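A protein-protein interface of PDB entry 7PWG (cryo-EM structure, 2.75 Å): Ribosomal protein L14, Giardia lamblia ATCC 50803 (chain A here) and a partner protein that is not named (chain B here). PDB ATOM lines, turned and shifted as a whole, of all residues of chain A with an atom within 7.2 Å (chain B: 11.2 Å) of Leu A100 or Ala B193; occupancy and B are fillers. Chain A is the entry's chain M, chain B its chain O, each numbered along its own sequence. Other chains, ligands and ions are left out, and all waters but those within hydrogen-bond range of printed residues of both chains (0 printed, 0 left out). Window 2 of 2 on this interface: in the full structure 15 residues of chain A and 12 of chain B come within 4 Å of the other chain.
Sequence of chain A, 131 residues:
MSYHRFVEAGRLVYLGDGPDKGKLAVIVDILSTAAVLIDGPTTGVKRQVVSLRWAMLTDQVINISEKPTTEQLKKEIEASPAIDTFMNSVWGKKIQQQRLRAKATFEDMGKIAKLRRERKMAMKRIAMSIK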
ATOM      1  N   ILE A  95      24.240  -2.559   6.781  1.00  0.00           N
ATOM      2  CA  ILE A  95      24.818  -2.293   5.466  1.00  0.00           C
ATOM      3  C   ILE A  95      23.809  -1.575   4.575  1.00  0.00           C
ATOM      4  O   ILE A  95      24.165  -0.664   3.819  1.00  0.00           O
ATOM      5  CB  ILE A  95      25.310  -3.607   4.828  1.00  0.00           C
ATOM      6  CG1 ILE A  95      26.773  -3.872   5.187  1.00  0.00           C
ATOM      7  CG2 ILE A  95      25.130  -3.594   3.316  1.00  0.00           C
ATOM      8  CD1 ILE A  95      27.208  -5.287   4.921  1.00  0.00           C
ATOM      9  N   GLN A  96      22.536  -1.957   4.667  1.00  0.00           N
ATOM     10  CA  GLN A  96      21.506  -1.293   3.877  1.00  0.00           C
ATOM     11  C   GLN A  96      21.421   0.190   4.205  1.00  0.00           C
ATOM     12  O   GLN A  96      21.346   1.028   3.301  1.00  0.00           O
ATOM     13  CB  GLN A  96      20.158  -1.969   4.101  1.00  0.00           C
ATOM     14  CG  GLN A  96      19.812  -3.011   3.056  1.00  0.00           C
ATOM     15  CD  GLN A  96      18.704  -3.930   3.510  1.00  0.00           C
ATOM     16  OE1 GLN A  96      17.815  -3.524   4.247  1.00  0.00           O
ATOM     17  NE2 GLN A  96      18.763  -5.185   3.086  1.00  0.00           N
ATOM     18  N   GLN A  97      21.429   0.541   5.493  1.00  0.00           N
ATOM     19  CA  GLN A  97      21.346   1.950   5.855  1.00  0.00           C
ATOM     20  C   GLN A  97      22.599   2.709   5.450  1.00  0.00           C
ATOM     21  O   GLN A  97      22.516   3.885   5.091  1.00  0.00           O
ATOM     22  CB  GLN A  97      21.094   2.131   7.351  1.00  0.00           C
ATOM     23  CG  GLN A  97      21.022   0.876   8.178  1.00  0.00           C
ATOM     24  CD  GLN A  97      20.761   1.165   9.655  1.00  0.00           C
ATOM     25  OE1 GLN A  97      20.879   0.284  10.504  1.00  0.00           O
ATOM     26  NE2 GLN A  97      20.396   2.397   9.960  1.00  0.00           N
ATOM     27  N   GLN A  98      23.760   2.061   5.472  1.00  0.00           N
ATOM     28  CA  GLN A  98      24.978   2.731   5.043  1.00  0.00           C
ATOM     29  C   GLN A  98      24.980   3.055   3.552  1.00  0.00           C
ATOM     30  O   GLN A  98      25.874   3.769   3.095  1.00  0.00           O
ATOM     31  CB  GLN A  98      26.199   1.882   5.404  1.00  0.00           C
ATOM     32  CG  GLN A  98      26.553   1.910   6.876  1.00  0.00           C
ATOM     33  CD  GLN A  98      27.577   0.865   7.261  1.00  0.00           C
ATOM     34  OE1 GLN A  98      27.967   0.032   6.447  1.00  0.00           O
ATOM     35  NE2 GLN A  98      28.016   0.901   8.512  1.00  0.00           N
ATOM     36  N   ARG A  99      24.031   2.535   2.784  1.00  0.00           N
ATOM     37  CA  ARG A  99      23.946   2.860   1.371  1.00  0.00           C
ATOM     38  C   ARG A  99      22.990   4.006   1.087  1.00  0.00           C
ATOM     39  O   ARG A  99      23.064   4.604   0.010  1.00  0.00           O
ATOM     40  CB  ARG A  99      23.534   1.623   0.574  1.00  0.00           C
ATOM     41  CG  ARG A  99      24.603   0.547   0.525  1.00  0.00           C
ATOM     42  CD  ARG A  99      24.054  -0.760   0.016  1.00  0.00           C
ATOM     43  NE  ARG A  99      25.094  -1.781  -0.098  1.00  0.00           N
ATOM     44  CZ  ARG A  99      24.860  -3.053  -0.400  1.00  0.00           C
ATOM     45  NH1 ARG A  99      23.619  -3.458  -0.610  1.00  0.00           N
ATOM     46  NH2 ARG A  99      25.859  -3.916  -0.483  1.00  0.00           N
ATOM     47  N   LEU A 100      22.107   4.332   2.024  1.00  0.00           N
ATOM     48  CA  LEU A 100      21.283   5.520   1.908  1.00  0.00           C
ATOM     49  C   LEU A 100      21.892   6.720   2.607  1.00  0.00           C
ATOM     50  O   LEU A 100      21.349   7.822   2.490  1.00  0.00           O
ATOM     51  CB  LEU A 100      19.885   5.266   2.473  1.00  0.00           C
ATOM     52  CG  LEU A 100      18.821   4.586   1.618  1.00  0.00           C
ATOM     53  CD1 LEU A 100      19.249   3.197   1.238  1.00  0.00           C
ATOM     54  CD2 LEU A 100      17.514   4.533   2.380  1.00  0.00           C
ATOM     55  N   ARG A 101      22.987   6.540   3.339  1.00  0.00           N
ATOM     56  CA  ARG A 101      23.683   7.653   3.969  1.00  0.00           C
ATOM     57  C   ARG A 101      25.018   7.933   3.300  1.00  0.00           C
ATOM     58  O   ARG A 101      25.816   8.714   3.827  1.00  0.00           O
ATOM     59  CB  ARG A 101      23.873   7.402   5.468  1.00  0.00           C
ATOM     60  CG  ARG A 101      24.823   6.286   5.799  1.00  0.00           C
ATOM     61  CD  ARG A 101      25.059   6.163   7.287  1.00  0.00           C
ATOM     62  NE  ARG A 101      23.910   5.634   7.999  1.00  0.00           N
ATOM     63  CZ  ARG A 101      23.974   5.024   9.179  1.00  0.00           C
ATOM     64  NH1 ARG A 101      25.133   4.849   9.787  1.00  0.00           N
ATOM     65  NH2 ARG A 101      22.869   4.585   9.751  1.00  0.00           N
ATOM     66  N   ALA A 102      25.278   7.320   2.151  1.00  0.00           N
ATOM     67  CA  ALA A 102      26.482   7.603   1.392  1.00  0.00           C
ATOM     68  C   ALA A 102      26.231   8.504   0.197  1.00  0.00           C
ATOM     69  O   ALA A 102      27.189   9.031  -0.373  1.00  0.00           O
ATOM     70  CB  ALA A 102      27.132   6.299   0.916  1.00  0.00           C
ATOM     71  N   LYS A 103      24.978   8.695  -0.194  1.00  0.00           N
ATOM     72  CA  LYS A 103      24.634   9.509  -1.347  1.00  0.00           C
ATOM     73  C   LYS A 103      24.348  10.961  -0.977  1.00  0.00           C
ATOM     74  O   LYS A 103      24.058  11.770  -1.864  1.00  0.00           O
ATOM     75  CB  LYS A 103      23.424   8.905  -2.058  1.00  0.00           C
ATOM     76  CG  LYS A 103      22.135   9.083  -1.284  1.00  0.00           C
ATOM     77  CD  LYS A 103      21.031   8.192  -1.828  1.00  0.00           C
ATOM     78  CE  LYS A 103      21.452   6.738  -1.814  1.00  0.00           C
ATOM     79  NZ  LYS A 103      20.441   5.857  -2.443  1.00  0.00           N
ATOM     80  N   ALA A 104      24.439  11.309   0.303  1.00  0.00           N
ATOM     81  CA  ALA A 104      23.904  12.573   0.792  1.00  0.00           C
ATOM     82  C   ALA A 104      24.653  13.769   0.221  1.00  0.00           C
ATOM     83  O   ALA A 104      25.861  13.717  -0.028  1.00  0.00           O
ATOM     84  CB  ALA A 104      23.950  12.620   2.317  1.00  0.00           C
ATOM     85  N   ILE A 112      19.526  16.364   7.960  1.00  0.00           N
ATOM     86  CA  ILE A 112      19.801  15.323   8.941  1.00  0.00           C
ATOM     87  C   ILE A 112      20.273  15.938  10.248  1.00  0.00           C
ATOM     88  O   ILE A 112      19.946  15.448  11.332  1.00  0.00           O
ATOM     89  CB  ILE A 112      20.833  14.326   8.381  1.00  0.00           C
ATOM     90  CG1 ILE A 112      20.418  13.853   6.995  1.00  0.00           C
ATOM     91  CG2 ILE A 112      20.957  13.133   9.276  1.00  0.00           C
ATOM     92  CD1 ILE A 112      21.520  13.183   6.241  1.00  0.00           C
ATOM     93  N   LEU B 185       8.011   9.379  17.081  1.00  0.00           N
ATOM     94  CA  LEU B 185       7.821   8.451  15.976  1.00  0.00           C
ATOM     95  C   LEU B 185       7.686   9.185  14.659  1.00  0.00           C
ATOM     96  O   LEU B 185       7.790   8.566  13.599  1.00  0.00           O
ATOM     97  CB  LEU B 185       6.600   7.569  16.226  1.00  0.00           C
ATOM     98  CG  LEU B 185       6.655   6.838  17.565  1.00  0.00           C
ATOM     99  CD1 LEU B 185       5.548   5.810  17.674  1.00  0.00           C
ATOM    100  CD2 LEU B 185       8.024   6.189  17.738  1.00  0.00           C
ATOM    101  N   GLN B 186       7.442  10.486  14.706  1.00  0.00           N
ATOM    102  CA  GLN B 186       7.557  11.309  13.521  1.00  0.00           C
ATOM    103  C   GLN B 186       8.995  11.740  13.280  1.00  0.00           C
ATOM    104  O   GLN B 186       9.349  12.063  12.144  1.00  0.00           O
ATOM    105  CB  GLN B 186       6.619  12.515  13.648  1.00  0.00           C
ATOM    106  CG  GLN B 186       7.270  13.810  14.086  1.00  0.00           C
ATOM    107  CD  GLN B 186       7.306  14.834  12.969  1.00  0.00           C
ATOM    108  OE1 GLN B 186       6.553  14.730  12.004  1.00  0.00           O
ATOM    109  NE2 GLN B 186       8.200  15.812  13.081  1.00  0.00           N
ATOM    110  N   ARG B 187       9.838  11.722  14.316  1.00  0.00           N
ATOM    111  CA  ARG B 187      11.257  12.012  14.137  1.00  0.00           C
ATOM    112  C   ARG B 187      12.032  10.802  13.625  1.00  0.00           C
ATOM    113  O   ARG B 187      12.894  10.946  12.759  1.00  0.00           O
ATOM    114  CB  ARG B 187      11.862  12.508  15.451  1.00  0.00           C
ATOM    115  CG  ARG B 187      11.685  13.986  15.690  1.00  0.00           C
ATOM    116  CD  ARG B 187      11.420  14.302  17.146  1.00  0.00           C
ATOM    117  NE  ARG B 187      10.910  15.663  17.290  1.00  0.00           N
ATOM    118  CZ  ARG B 187      10.499  16.222  18.429  1.00  0.00           C
ATOM    119  NH1 ARG B 187      10.528  15.543  19.570  1.00  0.00           N
ATOM    120  NH2 ARG B 187      10.050  17.475  18.423  1.00  0.00           N
ATOM    121  N   ILE B 188      11.739   9.606  14.136  1.00  0.00           N
ATOM    122  CA  ILE B 188      12.531   8.427  13.785  1.00  0.00           C
ATOM    123  C   ILE B 188      12.305   8.029  12.332  1.00  0.00           C
ATOM    124  O   ILE B 188      13.229   7.588  11.642  1.00  0.00           O
ATOM    125  CB  ILE B 188      12.209   7.268  14.742  1.00  0.00           C
ATOM    126  CG1 ILE B 188      12.498   7.671  16.181  1.00  0.00           C
ATOM    127  CG2 ILE B 188      13.024   6.031  14.402  1.00  0.00           C
ATOM    128  CD1 ILE B 188      13.808   8.318  16.365  1.00  0.00           C
ATOM    129  N   ASN B 189      11.076   8.167  11.848  1.00  0.00           N
ATOM    130  CA  ASN B 189      10.753   7.719  10.497  1.00  0.00           C
ATOM    131  C   ASN B 189      11.331   8.637   9.425  1.00  0.00           C
ATOM    132  O   ASN B 189      11.586   8.186   8.306  1.00  0.00           O
ATOM    133  CB  ASN B 189       9.244   7.603  10.353  1.00  0.00           C
ATOM    134  CG  ASN B 189       8.650   6.597  11.316  1.00  0.00           C
ATOM    135  OD1 ASN B 189       9.213   5.526  11.528  1.00  0.00           O
ATOM    136  ND2 ASN B 189       7.509   6.937  11.911  1.00  0.00           N
ATOM    137  N   ALA B 190      11.512   9.925   9.724  1.00  0.00           N
ATOM    138  CA  ALA B 190      12.190  10.801   8.776  1.00  0.00           C
ATOM    139  C   ALA B 190      13.690  10.543   8.772  1.00  0.00           C
ATOM    140  O   ALA B 190      14.324  10.539   7.712  1.00  0.00           O
ATOM    141  CB  ALA B 190      11.899  12.262   9.101  1.00  0.00           C
ATOM    142  N   GLU B 191      14.277  10.337   9.953  1.00  0.00           N
ATOM    143  CA  GLU B 191      15.650   9.868  10.016  1.00  0.00           C
ATOM    144  C   GLU B 191      15.824   8.525   9.334  1.00  0.00           C
ATOM    145  O   GLU B 191      16.943   8.187   8.942  1.00  0.00           O
ATOM    146  CB  GLU B 191      16.112   9.766  11.463  1.00  0.00           C
ATOM    147  CG  GLU B 191      16.344  11.092  12.158  1.00  0.00           C
ATOM    148  CD  GLU B 191      17.604  11.775  11.693  1.00  0.00           C
ATOM    149  OE1 GLU B 191      17.748  12.029  10.482  1.00  0.00           O
ATOM    150  OE2 GLU B 191      18.464  12.055  12.544  1.00  0.00           O
ATOM    151  N   LEU B 192      14.749   7.747   9.194  1.00  0.00           N
ATOM    152  CA  LEU B 192      14.851   6.448   8.540  1.00  0.00           C
ATOM    153  C   LEU B 192      15.202   6.587   7.068  1.00  0.00           C
ATOM    154  O   LEU B 192      15.998   5.805   6.540  1.00  0.00           O
ATOM    155  CB  LEU B 192      13.543   5.673   8.699  1.00  0.00           C
ATOM    156  CG  LEU B 192      13.521   4.742   9.914  1.00  0.00           C
ATOM    157  CD1 LEU B 192      12.534   3.598   9.734  1.00  0.00           C
ATOM    158  CD2 LEU B 192      14.933   4.220  10.229  1.00  0.00           C
ATOM    159  N   ALA B 193      14.602   7.562   6.388  1.00  0.00           N
ATOM    160  CA  ALA B 193      14.812   7.706   4.953  1.00  0.00           C
ATOM    161  C   ALA B 193      16.272   7.988   4.635  1.00  0.00           C
ATOM    162  O   ALA B 193      16.817   7.463   3.659  1.00  0.00           O
ATOM    163  CB  ALA B 193      13.930   8.826   4.414  1.00  0.00           C
ATOM    164  N   LYS B 194      16.915   8.821   5.440  1.00  0.00           N
ATOM    165  CA  LYS B 194      18.266   9.268   5.169  1.00  0.00           C
ATOM    166  C   LYS B 194      19.326   8.303   5.679  1.00  0.00           C
ATOM    167  O   LYS B 194      20.503   8.479   5.355  1.00  0.00           O
ATOM    168  CB  LYS B 194      18.484  10.651   5.789  1.00  0.00           C
ATOM    169  CG  LYS B 194      17.367  11.647   5.516  1.00  0.00           C
ATOM    170  CD  LYS B 194      17.497  12.261   4.132  1.00  0.00           C
ATOM    171  CE  LYS B 194      16.398  13.260   3.860  1.00  0.00           C
ATOM    172  NZ  LYS B 194      16.273  14.248   4.947  1.00  0.00           N
ATOM    173  N   TYR B 195      18.950   7.303   6.464  1.00  0.00           N
ATOM    174  CA  TYR B 195      19.917   6.351   6.997  1.00  0.00           C
ATOM    175  C   TYR B 195      19.952   5.121   6.126  1.00  0.00           C
ATOM    176  O   TYR B 195      19.010   4.859   5.382  1.00  0.00           O
ATOM    177  CB  TYR B 195      19.579   5.966   8.441  1.00  0.00           C
ATOM    178  CG  TYR B 195      19.827   7.059   9.450  1.00  0.00           C
ATOM    179  CD1 TYR B 195      20.721   8.079   9.185  1.00  0.00           C
ATOM    180  CD2 TYR B 195      19.175   7.066  10.665  1.00  0.00           C
ATOM    181  CE1 TYR B 195      20.965   9.067  10.084  1.00  0.00           C
ATOM    182  CE2 TYR B 195      19.406   8.059  11.579  1.00  0.00           C
ATOM    183  CZ  TYR B 195      20.303   9.061  11.282  1.00  0.00           C
ATOM    184  OH  TYR B 195      20.552  10.065  12.191  1.00  0.00           O
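Among the printed residues, pairs that only touch across the chains: Gln A97 with Tyr B195, Leu A100 with Ala B193, Leu A100 with Tyr B195, Arg A101 with Lys B194, Arg A101 with Tyr B195, Ile A112 with Glu B191 and Ile A112 with Lys B194.
Of chain A, only Leu A100 comes within 4 Å of Ala B193.
No residue of chain B comes within 4 Å of Ala A102.
No residue of chain B comes within 4 Å of Lys A103.
Printed residues of chain B within 4 Å of Arg A101: Lys B194 (3.5 Å) and Tyr B195 (3.8 Å).
Printed residues of chain B within 4 Å of Gln A97: Tyr B195.
Of the printed residues of chain A, Glu B191 touches Ile A112.
Of the printed residues of chain A, Tyr B195 touches Gln A97 (3.0 Å), Leu A100 (3.1 Å) and Arg A101 (3.8 Å).
Of the printed residues of chain B, Ile A112 touches Glu B191 (3.6 Å) and Lys B194 (3.9 Å).
Ile A95 touches none of the printed residues of chain B.
Arg B187 touches none of the printed residues of chain A.
The side-chain amide nitrogen of Gln A97 sits close to the guanidinium group of Arg A101 (3.3 Å).
OE2 of Glu B191 is in hydrogen-bond range of OH of Tyr B195 (2.9 Å).
The backbone carbonyl oxygen of Leu A100 sits close to the backbone carbonyl oxygen of Lys B194, at 3.1 Å.
Hydrophobic or aromatic side chains of chain B that line the printed part of chain A: Tyr B195.
Along chain B the printed residues that touch a printed residue of chain A span positions 191 to 195.
Printed residues of chain A that touch a printed residue of chain B: Gln A97, Leu A100, Arg A101 and Ile A112.
Among the printed residues, no Asp or Glu carboxylate lies within 4 Å of a Lys or Arg side-chain nitrogen of the other chain.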
